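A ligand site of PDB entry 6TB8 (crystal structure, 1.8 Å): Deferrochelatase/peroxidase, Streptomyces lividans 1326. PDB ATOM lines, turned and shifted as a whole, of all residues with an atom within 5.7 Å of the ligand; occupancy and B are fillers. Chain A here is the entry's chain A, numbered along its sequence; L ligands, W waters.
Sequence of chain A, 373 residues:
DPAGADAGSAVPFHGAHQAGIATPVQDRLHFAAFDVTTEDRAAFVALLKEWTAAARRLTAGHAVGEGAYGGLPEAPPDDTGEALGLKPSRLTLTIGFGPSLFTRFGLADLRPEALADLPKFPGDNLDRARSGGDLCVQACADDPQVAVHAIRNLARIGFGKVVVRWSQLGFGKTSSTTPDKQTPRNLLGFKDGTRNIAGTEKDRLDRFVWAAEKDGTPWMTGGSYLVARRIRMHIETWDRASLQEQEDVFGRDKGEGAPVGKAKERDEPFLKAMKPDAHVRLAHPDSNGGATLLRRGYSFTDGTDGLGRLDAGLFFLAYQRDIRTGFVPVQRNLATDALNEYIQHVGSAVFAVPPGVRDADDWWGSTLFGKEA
NE of Arg 195 lies within salt-bridge range of O3 of the ligand (2.8 Å).
O1 of the ligand is in hydrogen-bond range of N of Gly 193.
An oxygen (O1) of the ligand is in salt-bridge range of the guanidinium group (NH2) of Arg 295 (2.8 Å).
A ring nitrogen (NE2) of His 279 binds an iron atom (FE1) of the ligand.
The backbone NH (N) of Thr 194 is in hydrogen-bond range of an oxygen (O1) of the ligand (3.3 Å).
The backbone NH of Arg 195 is in hydrogen-bond range of an oxygen (O2) of the ligand (3.0 Å).
The side-chain amide oxygen of Asn 186 lies within hydrogen-bond range of the backbone NH of Leu 188, 3.0 Å away.
The guanidinium group of Arg 195 lies within hydrogen-bond range of a ring nitrogen (NE2) of His 284.
The backbone carbonyl oxygen (O) of Phe 250 sits close to the backbone NH (N) of Val 280.
ND2 of Asn 186 is in hydrogen-bond range of OD2 of Asp 192, at 2.8 Å.
The guanidinium group (NH1) of Arg 295 lies within salt-bridge range of the side-chain carboxylate (OD1) of Asp 192, at 3.1 Å.
O of Leu 293 sits close to OD1 of Asn 196 (3.4 Å).
O of Arg 195 lies within hydrogen-bond range of NH2 of Arg 295 (2.8 Å).
O of Ile 231 sits at hydrogen-bond distance from N of Leu 314, at 2.8 Å.
ND2 of Asn 186 touches C17 of the ligand (3.5 Å).
Leu 188 touches the ligand (CD1 to C17, 3.9 Å).
Phe 190 touches the ligand.
Lys 191 touches the ligand.
OD2 of Asp 192 touches C2 of the ligand, 3.4 Å away.
Ile 231 touches the ligand (CG2 to C19, 3.8 Å).
Met 233 touches the ligand.
CE1 of Phe 250 touches C2 of the ligand, 3.2 Å away.
Arg 252 touches the ligand.
CG1 of Val 280 touches O3 of the ligand, 3.6 Å away.
Ala 283 touches the ligand.
CD2 of His 284 touches O3 of the ligand (3.4 Å).
Pro 285 touches the ligand.
CD1 of Leu 293 touches C25 of the ligand, at 3.9 Å.
Leu 314 touches the ligand.
Phe 316 touches the ligand (CE2 to C21, 3.3 Å).
Phe 327 touches the ligand (CE1 to C26, 3.3 Å).
Val 330 touches the ligand.
Gln 331 touches the ligand (OE1 to C26, 3.5 Å).
Leu 334 touches the ligand (CD1 to C22, 3.9 Å).
CD2 of Leu 339 touches C15 of the ligand, 3.6 Å away.
Ile 343 touches the ligand (CG2 to C19, 3.9 Å).
Hydrophobic or aromatic side chains that line the ligand: Leu 188, Phe 190, Ile 231, Met 233, Phe 250, His 279, Val 280, Ala 283, His 284, Pro 285, Leu 293, Leu 314, Phe 316, Phe 327, Val 330, Leu 334, Leu 339 and Ile 343.
27 residues have an atom within 4 Å of the ligand: Asn 186, Leu 188, Phe 190, Lys 191, Asp 192, Gly 193, Thr 194, Arg 195, Ile 231, Met 233, Phe 250, Arg 252, His 279, Val 280, Ala 283, His 284, Pro 285, Leu 293, Arg 295, Leu 314, Phe 316, Phe 327, Val 330, Gln 331, Leu 334, Leu 339 and Ile 343.
The nearest printed residue that does not touch the ligand is His 345 (4.05 Å).
Water W2 bridges OD1 of Asp 192 (2.7 Å) and NH1 of Arg 295 (2.8 Å).
Water W1 bridges an oxygen (O2) of the ligand (2.7 Å) and the guanidinium group of Arg 252 (2.9 Å).
Water W5 lies within hydrogen-bond range of O4 of the ligand (2.7 Å) and O of Arg 195 (2.7 Å).
Water W6 bridges NE2 of His 345 (2.8 Å) and OE1 of Gln 331 (3.0 Å).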
ATOM      1  N   ASN A 186     -10.692  10.409   3.142  1.00  0.00           N
ATOM      2  CA  ASN A 186     -10.880  10.618   4.578  1.00  0.00           C
ATOM      3  C   ASN A 186     -11.090  12.099   4.848  1.00  0.00           C
ATOM      4  O   ASN A 186     -11.076  12.925   3.938  1.00  0.00           O
ATOM      5  CB  ASN A 186      -9.675  10.060   5.348  1.00  0.00           C
ATOM      6  CG  ASN A 186      -8.373  10.650   4.890  1.00  0.00           C
ATOM      7  OD1 ASN A 186      -8.287  11.856   4.631  1.00  0.00           O
ATOM      8  ND2 ASN A 186      -7.349   9.796   4.758  1.00  0.00           N
ATOM      9  N   LEU A 188      -9.252  14.308   6.140  1.00  0.00           N
ATOM     10  CA  LEU A 188      -8.138  15.189   5.802  1.00  0.00           C
ATOM     11  C   LEU A 188      -8.112  15.520   4.312  1.00  0.00           C
ATOM     12  O   LEU A 188      -7.239  16.271   3.869  1.00  0.00           O
ATOM     13  CB  LEU A 188      -6.804  14.579   6.219  1.00  0.00           C
ATOM     14  CG  LEU A 188      -6.618  14.188   7.698  1.00  0.00           C
ATOM     15  CD1 LEU A 188      -5.173  13.732   7.952  1.00  0.00           C
ATOM     16  CD2 LEU A 188      -7.067  15.308   8.602  1.00  0.00           C
ATOM     17  N   PHE A 190      -7.635  13.388   1.713  1.00  0.00           N
ATOM     18  CA  PHE A 190      -6.838  12.503   0.868  1.00  0.00           C
ATOM     19  C   PHE A 190      -7.537  11.173   0.595  1.00  0.00           C
ATOM     20  O   PHE A 190      -8.196  10.617   1.466  1.00  0.00           O
ATOM     21  CB  PHE A 190      -5.478  12.225   1.504  1.00  0.00           C
ATOM     22  CG  PHE A 190      -4.490  13.340   1.332  1.00  0.00           C
ATOM     23  CD1 PHE A 190      -4.639  14.539   2.017  1.00  0.00           C
ATOM     24  CD2 PHE A 190      -3.415  13.185   0.469  1.00  0.00           C
ATOM     25  CE1 PHE A 190      -3.724  15.579   1.874  1.00  0.00           C
ATOM     26  CE2 PHE A 190      -2.466  14.236   0.340  1.00  0.00           C
ATOM     27  CZ  PHE A 190      -2.629  15.415   1.023  1.00  0.00           C
ATOM     28  N   LYS A 191      -7.339  10.666  -0.610  1.00  0.00           N
ATOM     29  CA  LYS A 191      -7.731   9.303  -0.926  1.00  0.00           C
ATOM     30  C   LYS A 191      -7.056   8.338   0.039  1.00  0.00           C
ATOM     31  O   LYS A 191      -5.870   8.484   0.345  1.00  0.00           O
ATOM     32  CB  LYS A 191      -7.338   8.984  -2.362  1.00  0.00           C
ATOM     33  CG  LYS A 191      -8.088   9.776  -3.422  1.00  0.00           C
ATOM     34  CD  LYS A 191      -7.555   9.371  -4.805  1.00  0.00           C
ATOM     35  CE  LYS A 191      -8.344  10.020  -5.954  1.00  0.00           C
ATOM     36  NZ  LYS A 191      -7.677   9.846  -7.263  1.00  0.00           N
ATOM     37  N   ASP A 192      -7.826   7.359   0.500  1.00  0.00           N
ATOM     38  CA  ASP A 192      -7.397   6.420   1.537  1.00  0.00           C
ATOM     39  C   ASP A 192      -7.848   5.034   1.096  1.00  0.00           C
ATOM     40  O   ASP A 192      -9.056   4.746   1.091  1.00  0.00           O
ATOM     41  CB  ASP A 192      -8.013   6.818   2.900  1.00  0.00           C
ATOM     42  CG  ASP A 192      -7.176   6.380   4.097  1.00  0.00           C
ATOM     43  OD1 ASP A 192      -6.418   5.379   4.013  1.00  0.00           O
ATOM     44  OD2 ASP A 192      -7.290   7.045   5.162  1.00  0.00           O
ATOM     45  N   GLY A 193      -6.882   4.196   0.702  1.00  0.00           N
ATOM     46  CA  GLY A 193      -7.154   2.846   0.281  1.00  0.00           C
ATOM     47  C   GLY A 193      -6.554   2.468  -1.067  1.00  0.00           C
ATOM     48  O   GLY A 193      -6.738   1.341  -1.526  1.00  0.00           O
ATOM     49  N   THR A 194      -5.824   3.378  -1.702  1.00  0.00           N
ATOM     50  CA  THR A 194      -5.196   3.092  -3.004  1.00  0.00           C
ATOM     51  C   THR A 194      -4.407   1.779  -2.984  1.00  0.00           C
ATOM     52  O   THR A 194      -4.659   0.872  -3.799  1.00  0.00           O
ATOM     53  CB  THR A 194      -4.273   4.232  -3.396  1.00  0.00           C
ATOM     54  OG1 THR A 194      -5.009   5.453  -3.459  1.00  0.00           O
ATOM     55  CG2 THR A 194      -3.604   3.971  -4.778  1.00  0.00           C
ATOM     56  N   ARG A 195      -3.412   1.683  -2.110  1.00  0.00           N
ATOM     57  CA  ARG A 195      -2.548   0.504  -2.057  1.00  0.00           C
ATOM     58  C   ARG A 195      -2.952  -0.309  -0.825  1.00  0.00           C
ATOM     59  O   ARG A 195      -2.368  -0.186   0.255  1.00  0.00           O
ATOM     60  CB  ARG A 195      -1.057   0.896  -2.040  1.00  0.00           C
ATOM     61  CG  ARG A 195      -0.488   1.172  -3.438  1.00  0.00           C
ATOM     62  CD  ARG A 195       1.034   1.508  -3.412  1.00  0.00           C
ATOM     63  NE  ARG A 195       1.698   0.707  -2.405  1.00  0.00           N
ATOM     64  CZ  ARG A 195       1.947  -0.585  -2.529  1.00  0.00           C
ATOM     65  NH1 ARG A 195       2.514  -1.245  -1.536  1.00  0.00           N
ATOM     66  NH2 ARG A 195       1.629  -1.211  -3.659  1.00  0.00           N
ATOM     67  N   ASN A 196      -3.932  -1.167  -1.023  1.00  0.00           N
ATOM     68  CA  ASN A 196      -4.528  -1.985   0.026  1.00  0.00           C
ATOM     69  C   ASN A 196      -4.392  -3.437  -0.432  1.00  0.00           C
ATOM     70  O   ASN A 196      -3.365  -3.818  -1.022  1.00  0.00           O
ATOM     71  CB  ASN A 196      -5.969  -1.569   0.268  1.00  0.00           C
ATOM     72  CG  ASN A 196      -6.496  -2.000   1.627  1.00  0.00           C
ATOM     73  OD1 ASN A 196      -5.766  -2.005   2.591  1.00  0.00           O
ATOM     74  ND2 ASN A 196      -7.765  -2.368   1.695  1.00  0.00           N
ATOM     75  N   ILE A 231      -9.167   6.998  15.941  1.00  0.00           N
ATOM     76  CA  ILE A 231      -8.134   8.020  15.749  1.00  0.00           C
ATOM     77  C   ILE A 231      -8.821   9.375  15.581  1.00  0.00           C
ATOM     78  O   ILE A 231      -9.543   9.602  14.600  1.00  0.00           O
ATOM     79  CB  ILE A 231      -7.232   7.712  14.545  1.00  0.00           C
ATOM     80  CG1 ILE A 231      -6.727   6.266  14.640  1.00  0.00           C
ATOM     81  CG2 ILE A 231      -6.120   8.693  14.491  1.00  0.00           C
ATOM     82  CD1 ILE A 231      -5.782   5.842  13.490  1.00  0.00           C
ATOM     83  N   MET A 233      -8.779  13.277  14.721  1.00  0.00           N
ATOM     84  CA  MET A 233      -8.044  14.162  13.824  1.00  0.00           C
ATOM     85  C   MET A 233      -8.049  15.580  14.380  1.00  0.00           C
ATOM     86  O   MET A 233      -9.121  16.111  14.739  1.00  0.00           O
ATOM     87  CB  MET A 233      -8.642  14.152  12.416  1.00  0.00           C
ATOM     88  CG  MET A 233      -8.456  12.868  11.752  1.00  0.00           C
ATOM     89  SD  MET A 233      -9.467  12.781  10.270  1.00  0.00           S
ATOM     90  CE  MET A 233      -8.759  11.379   9.443  1.00  0.00           C
ATOM     91  N   PHE A 250       1.999  12.940   3.680  1.00  0.00           N
ATOM     92  CA  PHE A 250       1.619  11.632   3.166  1.00  0.00           C
ATOM     93  C   PHE A 250       2.586  11.075   2.122  1.00  0.00           C
ATOM     94  O   PHE A 250       2.781   9.866   2.068  1.00  0.00           O
ATOM     95  CB  PHE A 250       0.208  11.672   2.547  1.00  0.00           C
ATOM     96  CG  PHE A 250      -0.881  11.705   3.582  1.00  0.00           C
ATOM     97  CD1 PHE A 250      -1.083  10.629   4.432  1.00  0.00           C
ATOM     98  CD2 PHE A 250      -1.674  12.831   3.739  1.00  0.00           C
ATOM     99  CE1 PHE A 250      -2.067  10.681   5.447  1.00  0.00           C
ATOM    100  CE2 PHE A 250      -2.670  12.887   4.732  1.00  0.00           C
ATOM    101  CZ  PHE A 250      -2.860  11.818   5.577  1.00  0.00           C
ATOM    102  N   ARG A 252       1.931  11.705  -1.112  1.00  0.00           N
ATOM    103  CA  ARG A 252       1.116  11.749  -2.322  1.00  0.00           C
ATOM    104  C   ARG A 252       0.559  13.143  -2.478  1.00  0.00           C
ATOM    105  O   ARG A 252       0.392  13.878  -1.501  1.00  0.00           O
ATOM    106  CB  ARG A 252      -0.044  10.732  -2.292  1.00  0.00           C
ATOM    107  CG  ARG A 252       0.390   9.280  -2.414  1.00  0.00           C
ATOM    108  CD  ARG A 252      -0.778   8.325  -2.114  1.00  0.00           C
ATOM    109  NE  ARG A 252      -0.387   6.928  -2.254  1.00  0.00           N
ATOM    110  CZ  ARG A 252      -0.388   6.256  -3.402  1.00  0.00           C
ATOM    111  NH1 ARG A 252      -0.758   6.853  -4.521  1.00  0.00           N
ATOM    112  NH2 ARG A 252      -0.020   4.988  -3.429  1.00  0.00           N
ATOM    113  N   PRO A 269       4.659   3.904  -6.090  1.00  0.00           N
ATOM    114  CA  PRO A 269       5.493   4.939  -5.482  1.00  0.00           C
ATOM    115  C   PRO A 269       6.972   4.668  -5.678  1.00  0.00           C
ATOM    116  O   PRO A 269       7.406   3.521  -5.861  1.00  0.00           O
ATOM    117  CB  PRO A 269       5.120   4.892  -3.994  1.00  0.00           C
ATOM    118  CG  PRO A 269       4.556   3.518  -3.785  1.00  0.00           C
ATOM    119  CD  PRO A 269       3.862   3.164  -5.083  1.00  0.00           C
ATOM    120  N   HIS A 279       4.100   9.478   5.617  1.00  0.00           N
ATOM    121  CA  HIS A 279       3.257   8.375   6.072  1.00  0.00           C
ATOM    122  C   HIS A 279       3.384   7.152   5.171  1.00  0.00           C
ATOM    123  O   HIS A 279       3.554   6.023   5.652  1.00  0.00           O
ATOM    124  CB  HIS A 279       1.804   8.879   6.158  1.00  0.00           C
ATOM    125  CG  HIS A 279       0.830   7.847   6.576  1.00  0.00           C
ATOM    126  ND1 HIS A 279       0.771   7.370   7.869  1.00  0.00           N
ATOM    127  CD2 HIS A 279      -0.151   7.210   5.896  1.00  0.00           C
ATOM    128  CE1 HIS A 279      -0.177   6.453   7.954  1.00  0.00           C
ATOM    129  NE2 HIS A 279      -0.745   6.334   6.761  1.00  0.00           N
ATOM    130  N   VAL A 280       3.291   7.343   3.850  1.00  0.00           N
ATOM    131  CA  VAL A 280       3.283   6.233   2.907  1.00  0.00           C
ATOM    132  C   VAL A 280       4.635   5.536   2.901  1.00  0.00           C
ATOM    133  O   VAL A 280       4.715   4.311   2.845  1.00  0.00           O
ATOM    134  CB  VAL A 280       2.902   6.718   1.498  1.00  0.00           C
ATOM    135  CG1 VAL A 280       3.219   5.635   0.431  1.00  0.00           C
ATOM    136  CG2 VAL A 280       1.434   7.111   1.447  1.00  0.00           C
ATOM    137  N   ALA A 283       4.827   3.428   6.061  1.00  0.00           N
ATOM    138  CA  ALA A 283       3.808   2.381   6.175  1.00  0.00           C
ATOM    139  C   ALA A 283       3.922   1.301   5.118  1.00  0.00           C
ATOM    140  O   ALA A 283       3.366   0.219   5.292  1.00  0.00           O
ATOM    141  CB  ALA A 283       2.406   2.988   6.082  1.00  0.00           C
ATOM    142  N   HIS A 284       4.658   1.581   4.070  1.00  0.00           N
ATOM    143  CA  HIS A 284       4.770   0.685   2.927  1.00  0.00           C
ATOM    144  C   HIS A 284       5.336  -0.664   3.345  1.00  0.00           C
ATOM    145  O   HIS A 284       6.232  -0.736   4.188  1.00  0.00           O
ATOM    146  CB  HIS A 284       5.659   1.321   1.866  1.00  0.00           C
ATOM    147  CG  HIS A 284       5.566   0.696   0.514  1.00  0.00           C
ATOM    148  ND1 HIS A 284       6.223  -0.478   0.197  1.00  0.00           N
ATOM    149  CD2 HIS A 284       4.947   1.092  -0.625  1.00  0.00           C
ATOM    150  CE1 HIS A 284       5.995  -0.789  -1.063  1.00  0.00           C
ATOM    151  NE2 HIS A 284       5.221   0.147  -1.593  1.00  0.00           N
ATOM    152  N   PRO A 285       4.878  -1.756   2.740  1.00  0.00           N
ATOM    153  CA  PRO A 285       5.426  -3.075   3.094  1.00  0.00           C
ATOM    154  C   PRO A 285       6.948  -3.130   3.031  1.00  0.00           C
ATOM    155  O   PRO A 285       7.559  -3.793   3.879  1.00  0.00           O
ATOM    156  CB  PRO A 285       4.757  -3.996   2.071  1.00  0.00           C
ATOM    157  CG  PRO A 285       3.399  -3.329   1.829  1.00  0.00           C
ATOM    158  CD  PRO A 285       3.706  -1.860   1.849  1.00  0.00           C
ATOM    159  N   LEU A 293      -1.288  -5.017   5.074  1.00  0.00           N
ATOM    160  CA  LEU A 293      -2.565  -4.995   5.786  1.00  0.00           C
ATOM    161  C   LEU A 293      -3.718  -4.901   4.800  1.00  0.00           C
ATOM    162  O   LEU A 293      -3.577  -4.359   3.711  1.00  0.00           O
ATOM    163  CB  LEU A 293      -2.651  -3.777   6.716  1.00  0.00           C
ATOM    164  CG  LEU A 293      -1.448  -3.497   7.618  1.00  0.00           C
ATOM    165  CD1 LEU A 293      -1.654  -2.163   8.340  1.00  0.00           C
ATOM    166  CD2 LEU A 293      -1.221  -4.657   8.606  1.00  0.00           C
ATOM    167  N   ARG A 295      -6.772  -2.768   5.024  1.00  0.00           N
ATOM    168  CA  ARG A 295      -7.392  -1.663   5.779  1.00  0.00           C
ATOM    169  C   ARG A 295      -8.852  -1.544   5.351  1.00  0.00           C
ATOM    170  O   ARG A 295      -9.180  -1.752   4.190  1.00  0.00           O
ATOM    171  CB  ARG A 295      -6.632  -0.373   5.496  1.00  0.00           C
ATOM    172  CG  ARG A 295      -5.215  -0.414   6.038  1.00  0.00           C
ATOM    173  CD  ARG A 295      -4.327   0.725   5.530  1.00  0.00           C
ATOM    174  NE  ARG A 295      -4.036   0.637   4.108  1.00  0.00           N
ATOM    175  CZ  ARG A 295      -4.161   1.649   3.246  1.00  0.00           C
ATOM    176  NH1 ARG A 295      -4.606   2.859   3.622  1.00  0.00           N
ATOM    177  NH2 ARG A 295      -3.853   1.445   1.968  1.00  0.00           N
ATOM    178  N   LEU A 314     -11.174   9.112  12.343  1.00  0.00           N
ATOM    179  CA  LEU A 314     -11.147   7.955  11.459  1.00  0.00           C
ATOM    180  C   LEU A 314     -11.109   6.730  12.355  1.00  0.00           C
ATOM    181  O   LEU A 314     -10.264   6.645  13.252  1.00  0.00           O
ATOM    182  CB  LEU A 314      -9.945   8.029  10.509  1.00  0.00           C
ATOM    183  CG  LEU A 314      -9.877   6.988   9.398  1.00  0.00           C
ATOM    184  CD1 LEU A 314      -9.144   7.578   8.199  1.00  0.00           C
ATOM    185  CD2 LEU A 314      -9.223   5.719   9.904  1.00  0.00           C
ATOM    186  N   PHE A 316     -10.143   3.269  12.384  1.00  0.00           N
ATOM    187  CA  PHE A 316      -9.199   2.519  11.598  1.00  0.00           C
ATOM    188  C   PHE A 316      -9.379   1.053  11.910  1.00  0.00           C
ATOM    189  O   PHE A 316      -9.458   0.668  13.080  1.00  0.00           O
ATOM    190  CB  PHE A 316      -7.768   2.967  11.903  1.00  0.00           C
ATOM    191  CG  PHE A 316      -6.726   2.184  11.151  1.00  0.00           C
ATOM    192  CD1 PHE A 316      -6.192   1.029  11.700  1.00  0.00           C
ATOM    193  CD2 PHE A 316      -6.263   2.627   9.925  1.00  0.00           C
ATOM    194  CE1 PHE A 316      -5.207   0.315  11.014  1.00  0.00           C
ATOM    195  CE2 PHE A 316      -5.252   1.940   9.257  1.00  0.00           C
ATOM    196  CZ  PHE A 316      -4.743   0.767   9.783  1.00  0.00           C
ATOM    197  N   PHE A 327      -0.151  -5.237  11.849  1.00  0.00           N
ATOM    198  CA  PHE A 327      -0.322  -3.894  12.400  1.00  0.00           C
ATOM    199  C   PHE A 327       0.826  -3.464  13.300  1.00  0.00           C
ATOM    200  O   PHE A 327       1.212  -2.285  13.290  1.00  0.00           O
ATOM    201  CB  PHE A 327      -1.638  -3.826  13.207  1.00  0.00           C
ATOM    202  CG  PHE A 327      -1.868  -2.498  13.880  1.00  0.00           C
ATOM    203  CD1 PHE A 327      -2.436  -1.451  13.195  1.00  0.00           C
ATOM    204  CD2 PHE A 327      -1.538  -2.323  15.218  1.00  0.00           C
ATOM    205  CE1 PHE A 327      -2.646  -0.232  13.802  1.00  0.00           C
ATOM    206  CE2 PHE A 327      -1.766  -1.093  15.844  1.00  0.00           C
ATOM    207  CZ  PHE A 327      -2.316  -0.052  15.126  1.00  0.00           C
ATOM    208  N   VAL A 330       4.080  -2.202  11.559  1.00  0.00           N
ATOM    209  CA  VAL A 330       3.775  -0.975  10.824  1.00  0.00           C
ATOM    210  C   VAL A 330       3.592   0.204  11.782  1.00  0.00           C
ATOM    211  O   VAL A 330       4.215   1.260  11.622  1.00  0.00           O
ATOM    212  CB  VAL A 330       2.526  -1.166   9.934  1.00  0.00           C
ATOM    213  CG1 VAL A 330       2.223   0.127   9.226  1.00  0.00           C
ATOM    214  CG2 VAL A 330       2.780  -2.277   8.930  1.00  0.00           C
ATOM    215  N   GLN A 331       2.695   0.060  12.781  1.00  0.00           N
ATOM    216  CA  GLN A 331       2.455   1.151  13.717  1.00  0.00           C
ATOM    217  C   GLN A 331       3.723   1.546  14.476  1.00  0.00           C
ATOM    218  O   GLN A 331       3.960   2.736  14.718  1.00  0.00           O
ATOM    219  CB  GLN A 331       1.325   0.786  14.682  1.00  0.00           C
ATOM    220  CG  GLN A 331       0.991   1.837  15.721  1.00  0.00           C
ATOM    221  CD  GLN A 331       0.554   3.153  15.094  1.00  0.00           C
ATOM    222  OE1 GLN A 331      -0.113   3.182  14.081  1.00  0.00           O
ATOM    223  NE2 GLN A 331       0.915   4.265  15.735  1.00  0.00           N
ATOM    224  N   LEU A 334       5.527   3.840  12.385  1.00  0.00           N
ATOM    225  CA  LEU A 334       4.913   5.168  12.361  1.00  0.00           C
ATOM    226  C   LEU A 334       5.272   6.008  13.594  1.00  0.00           C
ATOM    227  O   LEU A 334       4.739   7.105  13.776  1.00  0.00           O
ATOM    228  CB  LEU A 334       3.383   5.044  12.237  1.00  0.00           C
ATOM    229  CG  LEU A 334       2.876   4.295  10.984  1.00  0.00           C
ATOM    230  CD1 LEU A 334       1.361   4.446  10.788  1.00  0.00           C
ATOM    231  CD2 LEU A 334       3.647   4.764   9.722  1.00  0.00           C
ATOM    232  N   LEU A 339       2.499  12.364  10.066  1.00  0.00           N
ATOM    233  CA  LEU A 339       1.061  12.436  10.351  1.00  0.00           C
ATOM    234  C   LEU A 339       0.773  12.587  11.845  1.00  0.00           C
ATOM    235  O   LEU A 339      -0.290  13.101  12.221  1.00  0.00           O
ATOM    236  CB  LEU A 339       0.336  11.200   9.803  1.00  0.00           C
ATOM    237  CG  LEU A 339      -1.203  11.128   9.975  1.00  0.00           C
ATOM    238  CD1 LEU A 339      -1.966  12.230   9.245  1.00  0.00           C
ATOM    239  CD2 LEU A 339      -1.624   9.747   9.506  1.00  0.00           C
ATOM    240  N   ILE A 343      -2.982  13.728  14.486  1.00  0.00           N
ATOM    241  CA  ILE A 343      -3.878  12.671  14.928  1.00  0.00           C
ATOM    242  C   ILE A 343      -3.555  12.313  16.379  1.00  0.00           C
ATOM    243  O   ILE A 343      -2.493  12.630  16.910  1.00  0.00           O
ATOM    244  CB  ILE A 343      -3.779  11.408  14.025  1.00  0.00           C
ATOM    245  CG1 ILE A 343      -2.379  10.786  14.135  1.00  0.00           C
ATOM    246  CG2 ILE A 343      -4.122  11.764  12.589  1.00  0.00           C
ATOM    247  CD1 ILE A 343      -2.264   9.443  13.460  1.00  0.00           C
ATOM    248  N   HIS A 345      -4.436   8.598  18.747  1.00  0.00           N
ATOM    249  CA  HIS A 345      -5.174   7.344  18.915  1.00  0.00           C
ATOM    250  C   HIS A 345      -5.848   7.407  20.272  1.00  0.00           C
ATOM    251  O   HIS A 345      -5.150   7.555  21.296  1.00  0.00           O
ATOM    252  CB  HIS A 345      -4.235   6.155  18.844  1.00  0.00           C
ATOM    253  CG  HIS A 345      -3.650   5.935  17.476  1.00  0.00           C
ATOM    254  ND1 HIS A 345      -3.791   4.754  16.806  1.00  0.00           N
ATOM    255  CD2 HIS A 345      -2.923   6.743  16.678  1.00  0.00           C
ATOM    256  CE1 HIS A 345      -3.177   4.826  15.640  1.00  0.00           C
ATOM    257  NE2 HIS A 345      -2.637   6.030  15.537  1.00  0.00           N
HETATM  258  C1  LIG L   1      -1.714   4.708   3.159  1.00  0.00           C
HETATM  259  C2  LIG L   1      -4.119   8.197   5.555  1.00  0.00           C
HETATM  260  C3  LIG L   1      -3.601   5.682   9.674  1.00  0.00           C
HETATM  261  C4  LIG L   1      -1.290   2.134   7.236  1.00  0.00           C
HETATM  262  C5  LIG L   1      -2.414   5.879   3.428  1.00  0.00           C
HETATM  263  C6  LIG L   1      -2.711   6.923   2.452  1.00  0.00           C
HETATM  264  C7  LIG L   1      -3.380   7.887   3.118  1.00  0.00           C
HETATM  265  C8  LIG L   1      -3.500   7.500   4.522  1.00  0.00           C
HETATM  266  C9  LIG L   1      -3.907   9.203   2.535  1.00  0.00           C
HETATM  267  C10 LIG L   1      -2.326   6.865   0.952  1.00  0.00           C
HETATM  268  C11 LIG L   1      -3.283   6.079   0.037  1.00  0.00           C
HETATM  269  C12 LIG L   1      -3.318   4.581   0.302  1.00  0.00           C
HETATM  270  O1  LIG L   1      -4.164   4.087   1.071  1.00  0.00           O
HETATM  271  O2  LIG L   1      -2.515   3.848  -0.291  1.00  0.00           O
HETATM  272  C13 LIG L   1      -4.191   7.811   6.877  1.00  0.00           C
HETATM  273  C14 LIG L   1      -4.850   8.562   7.947  1.00  0.00           C
HETATM  274  C15 LIG L   1      -4.717   7.882   9.095  1.00  0.00           C
HETATM  275  C16 LIG L   1      -3.953   6.675   8.791  1.00  0.00           C
HETATM  276  C17 LIG L   1      -5.523   9.897   7.687  1.00  0.00           C
HETATM  277  C18 LIG L   1      -5.238   8.235  10.488  1.00  0.00           C
HETATM  278  C19 LIG L   1      -6.222   9.123  10.711  1.00  0.00           C
HETATM  279  C20 LIG L   1      -2.902   4.519   9.347  1.00  0.00           C
HETATM  280  C21 LIG L   1      -2.511   3.501  10.291  1.00  0.00           C
HETATM  281  C22 LIG L   1      -1.876   2.515   9.637  1.00  0.00           C
HETATM  282  C23 LIG L   1      -1.838   2.892   8.257  1.00  0.00           C
HETATM  283  C24 LIG L   1      -2.826   3.606  11.796  1.00  0.00           C
HETATM  284  C25 LIG L   1      -1.234   1.228  10.174  1.00  0.00           C
HETATM  285  C26 LIG L   1      -0.810   1.086  11.425  1.00  0.00           C
HETATM  286  C27 LIG L   1      -1.246   2.529   5.924  1.00  0.00           C
HETATM  287  C28 LIG L   1      -0.672   1.762   4.839  1.00  0.00           C
HETATM  288  C29 LIG L   1      -0.780   2.463   3.722  1.00  0.00           C
HETATM  289  C30 LIG L   1      -1.433   3.712   4.062  1.00  0.00           C
HETATM  290  C31 LIG L   1      -0.095   0.357   5.029  1.00  0.00           C
HETATM  291  C32 LIG L   1      -0.361   1.997   2.311  1.00  0.00           C
HETATM  292  C33 LIG L   1       1.142   2.218   2.115  1.00  0.00           C
HETATM  293  C34 LIG L   1       1.591   1.604   0.805  1.00  0.00           C
HETATM  294  O3  LIG L   1       1.816   2.374  -0.159  1.00  0.00           O
HETATM  295  O4  LIG L   1       1.728   0.367   0.715  1.00  0.00           O
HETATM  296  N1  LIG L   1      -2.897   6.258   4.664  1.00  0.00           N
HETATM  297  N2  LIG L   1      -3.684   6.678   7.442  1.00  0.00           N
HETATM  298  N3  LIG L   1      -2.497   4.105   8.102  1.00  0.00           N
HETATM  299  N4  LIG L   1      -1.700   3.723   5.416  1.00  0.00           N
HETATM  300 FE1  LIG L   1      -2.605   5.242   6.391  1.00  0.00          FE
HETATM  301  O   HOH W   1       0.015   4.621  -0.571  1.00  0.00           O
HETATM  302  O   HOH W   2      -4.716   4.427   5.912  1.00  0.00           O
HETATM  303  O   HOH W   3      -0.288  -2.762   3.623  1.00  0.00           O
HETATM  304  O   HOH W   4       1.920  -2.242   5.214  1.00  0.00           O
HETATM  305  O   HOH W   5      -0.120  -1.572   0.988  1.00  0.00           O
HETATM  306  O   HOH W   6      -0.896   5.941  13.309  1.00  0.00           O
HETATM  307  O   HOH W   7      -6.820   5.549   7.318  1.00  0.00           O
